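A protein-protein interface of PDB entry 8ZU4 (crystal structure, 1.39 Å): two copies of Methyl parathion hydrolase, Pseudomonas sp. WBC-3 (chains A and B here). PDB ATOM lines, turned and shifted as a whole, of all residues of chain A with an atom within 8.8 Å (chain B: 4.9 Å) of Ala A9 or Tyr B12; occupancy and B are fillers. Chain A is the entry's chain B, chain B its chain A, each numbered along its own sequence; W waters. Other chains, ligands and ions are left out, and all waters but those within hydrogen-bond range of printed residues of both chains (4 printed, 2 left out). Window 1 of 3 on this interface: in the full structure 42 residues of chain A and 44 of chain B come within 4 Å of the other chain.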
ATOM      1  N   VAL A   5      11.070  10.021  17.252  1.00  0.00           N
ATOM      2  CA  VAL A   5      11.059   9.702  15.833  1.00  0.00           C
ATOM      3  C   VAL A   5      12.475   9.598  15.274  1.00  0.00           C
ATOM      4  O   VAL A   5      12.812   8.631  14.589  1.00  0.00           O
ATOM      5  CB  VAL A   5      10.197  10.739  15.078  1.00  0.00           C
ATOM      6  CG1 VAL A   5      10.180  10.460  13.594  1.00  0.00           C
ATOM      7  CG2 VAL A   5       8.779  10.742  15.644  1.00  0.00           C
ATOM      8  N   ARG A   6      13.317  10.587  15.579  1.00  0.00           N
ATOM      9  CA  ARG A   6      14.757  10.549  15.291  1.00  0.00           C
ATOM     10  C   ARG A   6      15.067  10.373  13.806  1.00  0.00           C
ATOM     11  O   ARG A   6      15.997   9.658  13.430  1.00  0.00           O
ATOM     12  CB  ARG A   6      15.484   9.506  16.146  1.00  0.00           C
ATOM     13  CG  ARG A   6      15.891  10.020  17.518  1.00  0.00           C
ATOM     14  CD  ARG A   6      16.825   9.064  18.233  1.00  0.00           C
ATOM     15  NE  ARG A   6      16.885   9.362  19.659  1.00  0.00           N
ATOM     16  CZ  ARG A   6      18.004   9.451  20.364  1.00  0.00           C
ATOM     17  NH1 ARG A   6      19.185   9.187  19.826  1.00  0.00           N
ATOM     18  NH2 ARG A   6      17.936   9.813  21.643  1.00  0.00           N
ATOM     19  N   THR A   7      14.299  11.040  12.949  1.00  0.00           N
ATOM     20  CA  THR A   7      14.588  11.091  11.522  1.00  0.00           C
ATOM     21  C   THR A   7      14.655  12.543  11.066  1.00  0.00           C
ATOM     22  O   THR A   7      13.935  13.401  11.583  1.00  0.00           O
ATOM     23  CB  THR A   7      13.546  10.318  10.693  1.00  0.00           C
ATOM     24  OG1 THR A   7      12.236  10.848  10.939  1.00  0.00           O
ATOM     25  CG2 THR A   7      13.572   8.843  11.041  1.00  0.00           C
ATOM     26  N   SER A   8      15.532  12.818  10.112  1.00  0.00           N
ATOM     27  CA  SER A   8      15.613  14.169   9.586  1.00  0.00           C
ATOM     28  C   SER A   8      14.551  14.385   8.508  1.00  0.00           C
ATOM     29  O   SER A   8      14.043  13.441   7.893  1.00  0.00           O
ATOM     30  CB  SER A   8      17.009  14.446   9.031  1.00  0.00           C
ATOM     31  OG  SER A   8      17.966  14.497  10.077  1.00  0.00           O
ATOM     32  N   ALA A   9      14.217  15.656   8.289  1.00  0.00           N
ATOM     33  CA  ALA A   9      13.280  16.019   7.242  1.00  0.00           C
ATOM     34  C   ALA A   9      13.895  15.714   5.878  1.00  0.00           C
ATOM     35  O   ALA A   9      15.114  15.558   5.760  1.00  0.00           O
ATOM     36  CB  ALA A   9      12.961  17.509   7.331  1.00  0.00           C
ATOM     37  N   PRO A  10      13.068  15.591   4.836  1.00  0.00           N
ATOM     38  CA  PRO A  10      13.614  15.341   3.495  1.00  0.00           C
ATOM     39  C   PRO A  10      14.625  16.412   3.114  1.00  0.00           C
ATOM     40  O   PRO A  10      14.413  17.605   3.343  1.00  0.00           O
ATOM     41  CB  PRO A  10      12.378  15.395   2.593  1.00  0.00           C
ATOM     42  CG  PRO A  10      11.239  15.060   3.495  1.00  0.00           C
ATOM     43  CD  PRO A  10      11.594  15.571   4.853  1.00  0.00           C
ATOM     44  N   GLY A  11      15.733  15.970   2.532  1.00  0.00           N
ATOM     45  CA  GLY A  11      16.868  16.840   2.315  1.00  0.00           C
ATOM     46  C   GLY A  11      16.821  17.596   1.009  1.00  0.00           C
ATOM     47  O   GLY A  11      17.645  17.372   0.115  1.00  0.00           O
ATOM     48  N   TYR A  12      15.840  18.481   0.873  1.00  0.00           N
ATOM     49  CA  TYR A  12      15.798  19.389  -0.259  1.00  0.00           C
ATOM     50  C   TYR A  12      15.443  20.788   0.213  1.00  0.00           C
ATOM     51  O   TYR A  12      14.693  20.975   1.180  1.00  0.00           O
ATOM     52  CB  TYR A  12      14.889  18.928  -1.411  1.00  0.00           C
ATOM     53  CG  TYR A  12      13.403  18.934  -1.119  1.00  0.00           C
ATOM     54  CD1 TYR A  12      12.804  17.871  -0.459  1.00  0.00           C
ATOM     55  CD2 TYR A  12      12.600  20.008  -1.503  1.00  0.00           C
ATOM     56  CE1 TYR A  12      11.440  17.854  -0.211  1.00  0.00           C
ATOM     57  CE2 TYR A  12      11.236  20.009  -1.245  1.00  0.00           C
ATOM     58  CZ  TYR A  12      10.664  18.927  -0.600  1.00  0.00           C
ATOM     59  OH  TYR A  12       9.309  18.907  -0.333  1.00  0.00           O
ATOM     60  N   SER A  26      20.273  17.233  -0.808  1.00  0.00           N
ATOM     61  CA  SER A  26      21.271  16.640   0.068  1.00  0.00           C
ATOM     62  C   SER A  26      21.534  15.197  -0.339  1.00  0.00           C
ATOM     63  O   SER A  26      20.597  14.426  -0.591  1.00  0.00           O
ATOM     64  CB  SER A  26      20.804  16.677   1.519  1.00  0.00           C
ATOM     65  OG  SER A  26      21.805  16.107   2.350  1.00  0.00           O
ATOM     66  N   ARG A  90      21.776   9.772  -0.630  1.00  0.00           N
ATOM     67  CA  ARG A  90      20.396  10.200  -0.452  1.00  0.00           C
ATOM     68  C   ARG A  90      19.860  11.039  -1.602  1.00  0.00           C
ATOM     69  O   ARG A  90      18.660  11.347  -1.607  1.00  0.00           O
ATOM     70  CB  ARG A  90      20.244  11.017   0.838  1.00  0.00           C
ATOM     71  CG  ARG A  90      20.870  10.404   2.080  1.00  0.00           C
ATOM     72  CD  ARG A  90      19.986   9.309   2.660  1.00  0.00           C
ATOM     73  NE  ARG A  90      20.541   8.739   3.883  1.00  0.00           N
ATOM     74  CZ  ARG A  90      21.514   7.838   3.924  1.00  0.00           C
ATOM     75  NH1 ARG A  90      22.081   7.382   2.820  1.00  0.00           N
ATOM     76  NH2 ARG A  90      21.926   7.381   5.105  1.00  0.00           N
ATOM     77  N   ASN A  94      15.945  12.300  -2.448  1.00  0.00           N
ATOM     78  CA  ASN A  94      15.582  13.692  -2.206  1.00  0.00           C
ATOM     79  C   ASN A  94      15.134  14.391  -3.482  1.00  0.00           C
ATOM     80  O   ASN A  94      14.283  15.278  -3.426  1.00  0.00           O
ATOM     81  CB  ASN A  94      16.705  14.435  -1.488  1.00  0.00           C
ATOM     82  CG  ASN A  94      16.826  14.015  -0.033  1.00  0.00           C
ATOM     83  OD1 ASN A  94      15.814  13.776   0.638  1.00  0.00           O
ATOM     84  ND2 ASN A  94      18.053  13.904   0.458  1.00  0.00           N
ATOM     85  N   ALA A  97      11.597  13.331  -3.540  1.00  0.00           N
ATOM     86  CA  ALA A  97      10.832  14.070  -2.539  1.00  0.00           C
ATOM     87  C   ALA A  97      10.603  15.513  -2.969  1.00  0.00           C
ATOM     88  O   ALA A  97       9.557  16.098  -2.656  1.00  0.00           O
ATOM     89  CB  ALA A  97      11.542  14.020  -1.188  1.00  0.00           C
ATOM     90  N   PHE A 270      24.571  22.152   4.438  1.00  0.00           N
ATOM     91  CA  PHE A 270      23.384  22.119   3.599  1.00  0.00           C
ATOM     92  C   PHE A 270      22.403  23.202   4.050  1.00  0.00           C
ATOM     93  O   PHE A 270      22.177  23.368   5.257  1.00  0.00           O
ATOM     94  CB  PHE A 270      22.729  20.735   3.704  1.00  0.00           C
ATOM     95  CG  PHE A 270      21.459  20.607   2.915  1.00  0.00           C
ATOM     96  CD1 PHE A 270      21.501  20.374   1.544  1.00  0.00           C
ATOM     97  CD2 PHE A 270      20.223  20.734   3.534  1.00  0.00           C
ATOM     98  CE1 PHE A 270      20.333  20.275   0.804  1.00  0.00           C
ATOM     99  CE2 PHE A 270      19.050  20.632   2.794  1.00  0.00           C
ATOM    100  CZ  PHE A 270      19.112  20.396   1.434  1.00  0.00           C
ATOM    101  N   TYR A 290      16.271  31.723   5.483  1.00  0.00           N
ATOM    102  CA  TYR A 290      15.198  30.791   5.157  1.00  0.00           C
ATOM    103  C   TYR A 290      14.037  31.517   4.489  1.00  0.00           C
ATOM    104  O   TYR A 290      13.525  32.519   5.000  1.00  0.00           O
ATOM    105  CB  TYR A 290      14.702  30.109   6.429  1.00  0.00           C
ATOM    106  CG  TYR A 290      13.545  29.161   6.189  1.00  0.00           C
ATOM    107  CD1 TYR A 290      13.742  27.920   5.594  1.00  0.00           C
ATOM    108  CD2 TYR A 290      12.253  29.510   6.555  1.00  0.00           C
ATOM    109  CE1 TYR A 290      12.679  27.056   5.380  1.00  0.00           C
ATOM    110  CE2 TYR A 290      11.189  28.660   6.349  1.00  0.00           C
ATOM    111  CZ  TYR A 290      11.404  27.432   5.763  1.00  0.00           C
ATOM    112  OH  TYR A 290      10.340  26.585   5.551  1.00  0.00           O
ATOM    113  N   PRO B  10       8.989  20.142   3.929  1.00  0.00           N
ATOM    114  CA  PRO B  10       8.286  20.212   5.217  1.00  0.00           C
ATOM    115  C   PRO B  10       9.124  20.954   6.247  1.00  0.00           C
ATOM    116  O   PRO B  10      10.337  20.758   6.357  1.00  0.00           O
ATOM    117  CB  PRO B  10       8.091  18.743   5.602  1.00  0.00           C
ATOM    118  CG  PRO B  10       8.184  17.986   4.320  1.00  0.00           C
ATOM    119  CD  PRO B  10       9.109  18.758   3.430  1.00  0.00           C
ATOM    120  N   GLY B  11       8.467  21.836   6.991  1.00  0.00           N
ATOM    121  CA  GLY B  11       9.182  22.754   7.851  1.00  0.00           C
ATOM    122  C   GLY B  11       9.434  22.193   9.231  1.00  0.00           C
ATOM    123  O   GLY B  11       8.871  22.677  10.216  1.00  0.00           O
ATOM    124  N   TYR B  12      10.252  21.148   9.318  1.00  0.00           N
ATOM    125  CA  TYR B  12      10.732  20.667  10.604  1.00  0.00           C
ATOM    126  C   TYR B  12      12.219  20.369  10.505  1.00  0.00           C
ATOM    127  O   TYR B  12      12.723  19.977   9.448  1.00  0.00           O
ATOM    128  CB  TYR B  12       9.953  19.469  11.157  1.00  0.00           C
ATOM    129  CG  TYR B  12      10.041  18.190  10.348  1.00  0.00           C
ATOM    130  CD1 TYR B  12       9.220  17.982   9.242  1.00  0.00           C
ATOM    131  CD2 TYR B  12      10.919  17.173  10.713  1.00  0.00           C
ATOM    132  CE1 TYR B  12       9.287  16.800   8.512  1.00  0.00           C
ATOM    133  CE2 TYR B  12      10.998  15.990   9.986  1.00  0.00           C
ATOM    134  CZ  TYR B  12      10.178  15.809   8.893  1.00  0.00           C
ATOM    135  OH  TYR B  12      10.260  14.628   8.184  1.00  0.00           O
ATOM    136  N   TYR B  13      12.917  20.588  11.616  1.00  0.00           N
ATOM    137  CA  TYR B  13      14.357  20.365  11.692  1.00  0.00           C
ATOM    138  C   TYR B  13      14.670  19.556  12.943  1.00  0.00           C
ATOM    139  O   TYR B  13      14.429  20.022  14.059  1.00  0.00           O
ATOM    140  CB  TYR B  13      15.121  21.693  11.712  1.00  0.00           C
ATOM    141  CG  TYR B  13      16.616  21.491  11.710  1.00  0.00           C
ATOM    142  CD1 TYR B  13      17.297  21.264  10.523  1.00  0.00           C
ATOM    143  CD2 TYR B  13      17.344  21.505  12.891  1.00  0.00           C
ATOM    144  CE1 TYR B  13      18.659  21.063  10.512  1.00  0.00           C
ATOM    145  CE2 TYR B  13      18.715  21.304  12.891  1.00  0.00           C
ATOM    146  CZ  TYR B  13      19.367  21.084  11.693  1.00  0.00           C
ATOM    147  OH  TYR B  13      20.731  20.881  11.656  1.00  0.00           O
ATOM    148  N   ARG B  14      15.216  18.356  12.763  1.00  0.00           N
ATOM    149  CA  ARG B  14      15.493  17.468  13.886  1.00  0.00           C
ATOM    150  C   ARG B  14      16.925  17.633  14.389  1.00  0.00           C
ATOM    151  O   ARG B  14      17.872  17.751  13.600  1.00  0.00           O
ATOM    152  CB  ARG B  14      15.284  16.009  13.474  1.00  0.00           C
ATOM    153  CG  ARG B  14      15.044  15.070  14.637  1.00  0.00           C
ATOM    154  CD  ARG B  14      13.560  15.014  14.961  1.00  0.00           C
ATOM    155  NE  ARG B  14      12.824  14.350  13.892  1.00  0.00           N
ATOM    156  CZ  ARG B  14      11.505  14.223  13.848  1.00  0.00           C
ATOM    157  NH1 ARG B  14      10.729  14.743  14.786  1.00  0.00           N
ATOM    158  NH2 ARG B  14      10.950  13.550  12.842  1.00  0.00           N
ATOM    159  N   THR B  23      12.783  19.095  17.877  1.00  0.00           N
ATOM    160  CA  THR B  23      12.281  19.323  16.528  1.00  0.00           C
ATOM    161  C   THR B  23      11.852  20.778  16.429  1.00  0.00           C
ATOM    162  O   THR B  23      10.872  21.184  17.062  1.00  0.00           O
ATOM    163  CB  THR B  23      11.127  18.378  16.196  1.00  0.00           C
ATOM    164  OG1 THR B  23      11.488  17.037  16.553  1.00  0.00           O
ATOM    165  CG2 THR B  23      10.816  18.437  14.698  1.00  0.00           C
ATOM    166  N   ALA B  24      12.599  21.564  15.666  1.00  0.00           N
ATOM    167  CA  ALA B  24      12.137  22.906  15.335  1.00  0.00           C
ATOM    168  C   ALA B  24      10.983  22.779  14.352  1.00  0.00           C
ATOM    169  O   ALA B  24      11.080  22.038  13.366  1.00  0.00           O
ATOM    170  CB  ALA B  24      13.275  23.719  14.722  1.00  0.00           C
ATOM    171  N   LEU B  25       9.886  23.479  14.624  1.00  0.00           N
ATOM    172  CA  LEU B  25       8.677  23.398  13.818  1.00  0.00           C
ATOM    173  C   LEU B  25       8.366  24.774  13.256  1.00  0.00           C
ATOM    174  O   LEU B  25       8.092  25.713  14.014  1.00  0.00           O
ATOM    175  CB  LEU B  25       7.489  22.876  14.631  1.00  0.00           C
ATOM    176  CG  LEU B  25       7.654  21.512  15.301  1.00  0.00           C
ATOM    177  CD1 LEU B  25       6.502  21.236  16.269  1.00  0.00           C
ATOM    178  CD2 LEU B  25       7.765  20.419  14.251  1.00  0.00           C
ATOM    179  N   ASN B  94       3.320  20.778  10.309  1.00  0.00           N
ATOM    180  CA  ASN B  94       4.721  20.385  10.399  1.00  0.00           C
ATOM    181  C   ASN B  94       4.968  19.465  11.589  1.00  0.00           C
ATOM    182  O   ASN B  94       5.832  18.586  11.523  1.00  0.00           O
ATOM    183  CB  ASN B  94       5.610  21.626  10.424  1.00  0.00           C
ATOM    184  CG  ASN B  94       5.728  22.265   9.060  1.00  0.00           C
ATOM    185  OD1 ASN B  94       5.810  21.566   8.040  1.00  0.00           O
ATOM    186  ND2 ASN B  94       5.727  23.594   9.024  1.00  0.00           N
ATOM    187  N   ALA B  97       4.015  16.264  10.144  1.00  0.00           N
ATOM    188  CA  ALA B  97       5.062  15.812   9.237  1.00  0.00           C
ATOM    189  C   ALA B  97       6.281  15.315   9.998  1.00  0.00           C
ATOM    190  O   ALA B  97       6.967  14.393   9.540  1.00  0.00           O
ATOM    191  CB  ALA B  97       5.453  16.934   8.271  1.00  0.00           C
ATOM    192  N   ALA B  98       6.556  15.896  11.165  1.00  0.00           N
ATOM    193  CA  ALA B  98       7.662  15.456  12.005  1.00  0.00           C
ATOM    194  C   ALA B  98       7.368  14.149  12.721  1.00  0.00           C
ATOM    195  O   ALA B  98       8.201  13.701  13.515  1.00  0.00           O
ATOM    196  CB  ALA B  98       8.019  16.536  13.030  1.00  0.00           C
ATOM    197  N   PHE B 270      14.722  30.128  10.312  1.00  0.00           N
ATOM    198  CA  PHE B 270      14.462  28.727  10.619  1.00  0.00           C
ATOM    199  C   PHE B 270      15.674  27.871  10.251  1.00  0.00           C
ATOM    200  O   PHE B 270      16.249  28.041   9.167  1.00  0.00           O
ATOM    201  CB  PHE B 270      13.233  28.253   9.833  1.00  0.00           C
ATOM    202  CG  PHE B 270      12.835  26.834  10.128  1.00  0.00           C
ATOM    203  CD1 PHE B 270      12.145  26.516  11.291  1.00  0.00           C
ATOM    204  CD2 PHE B 270      13.170  25.814   9.248  1.00  0.00           C
ATOM    205  CE1 PHE B 270      11.791  25.201  11.572  1.00  0.00           C
ATOM    206  CE2 PHE B 270      12.818  24.492   9.526  1.00  0.00           C
ATOM    207  CZ  PHE B 270      12.130  24.189  10.683  1.00  0.00           C
ATOM    208  N   TYR B 290      24.397  21.781   9.691  1.00  0.00           N
ATOM    209  CA  TYR B 290      23.425  20.767   9.291  1.00  0.00           C
ATOM    210  C   TYR B 290      23.918  19.384   9.704  1.00  0.00           C
ATOM    211  O   TYR B 290      25.044  18.988   9.399  1.00  0.00           O
ATOM    212  CB  TYR B 290      23.197  20.804   7.776  1.00  0.00           C
ATOM    213  CG  TYR B 290      22.251  19.715   7.303  1.00  0.00           C
ATOM    214  CD1 TYR B 290      20.877  19.834   7.493  1.00  0.00           C
ATOM    215  CD2 TYR B 290      22.728  18.571   6.672  1.00  0.00           C
ATOM    216  CE1 TYR B 290      20.009  18.842   7.080  1.00  0.00           C
ATOM    217  CE2 TYR B 290      21.863  17.569   6.245  1.00  0.00           C
ATOM    218  CZ  TYR B 290      20.498  17.715   6.454  1.00  0.00           C
ATOM    219  OH  TYR B 290      19.619  16.735   6.041  1.00  0.00           O
HETATM  220  O   HOH W   1      17.072  17.272   6.318  1.00  0.00           O
HETATM  221  O   HOH W   2      20.557  14.702   4.343  1.00  0.00           O
HETATM  222  O   HOH W   3      18.306  17.069  11.006  1.00  0.00           O
HETATM  223  O   HOH W   4      15.962  17.731   9.727  1.00  0.00           O
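The backbone carbonyl oxygen of Thr A7 is in hydrogen-bond range of the guanidinium group of Arg B14 (2.7 Å).
Among the printed residues, pairs that only touch across the chains: Val A5 with Arg B14 (3.3 Å), Val A5 with Ala B98 (3.7 Å), Ser A8 with Tyr B12 (3.98 Å), Ala A9 with Tyr B12 (3.3 Å), Pro A10 with Tyr B12 (3.7 Å), Tyr A12 with Pro B10 (3.8 Å), Phe A270 with Tyr B290 (3.7 Å) and Tyr A290 with Phe B270 (3.6 Å).
Pro A10 touches Tyr B12, and with the chains exchanged Tyr A12 touches Pro B10. Phe A270 touches Tyr B290, and with the chains exchanged Tyr A290 touches Phe B270.
Water W1 lies within hydrogen-bond range of the side-chain hydroxyl of Tyr B290 and the backbone carbonyl oxygen of Ala A9. Water W3 lies within hydrogen-bond range of the backbone carbonyl oxygen of Arg B14 (2.7 Å) and the side-chain hydroxyl of Ser A8 (2.8 Å). Water W2 bridges the side-chain hydroxyl of Ser A26 and the side-chain hydroxyl of Tyr B290. Water W4 bridges the backbone NH of Ala A9 (3.1 Å) and the backbone NH of Arg B14 (3.2 Å).
Of the 14 printed residues of chain A, 8 touch a printed residue of chain B. Hydrophobic or aromatic side chains of chain A that line the printed part of chain B: Val A5, Ala A9, Pro A10, Tyr A12, Phe A270 and Tyr A290. Printed residues of chain B that touch a printed residue of chain A: Pro B10, Tyr B12, Arg B14, Ala B98, Phe B270 and Tyr B290. Hydrophobic or aromatic side chains of chain B within 4 Å of the printed part of chain A: Pro B10, Tyr B12, Phe B270 and Tyr B290.
OG1 of Thr B23 sits at hydrogen-bond distance from NH1 of Arg B14. O of Ala B98 sits at hydrogen-bond distance from NH2 of Arg B14 (2.8 Å).
Arg A6 touches none of the printed residues of chain B. Ala A9 touches just one residue of chain B: Tyr B12. Printed residues of chain B within 4 Å of Pro A10: Tyr B12. Printed residues of chain B within 4 Å of Phe A270: Tyr B290 (3.7 Å). Of the printed residues of chain A, Arg B14 touches Val A5 (3.3 Å) and Thr A7 (2.7 Å). Thr B23 touches none of the printed residues of chain A. Printed residues of chain A within 4 Å of Ala B98: Val A5 (3.7 Å). Of the printed residues of chain A, Phe B270 touches Tyr A290 (3.6 Å). The nearest residue of chain A that does not touch Tyr B12 is Thr A7 (4.2 Å).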
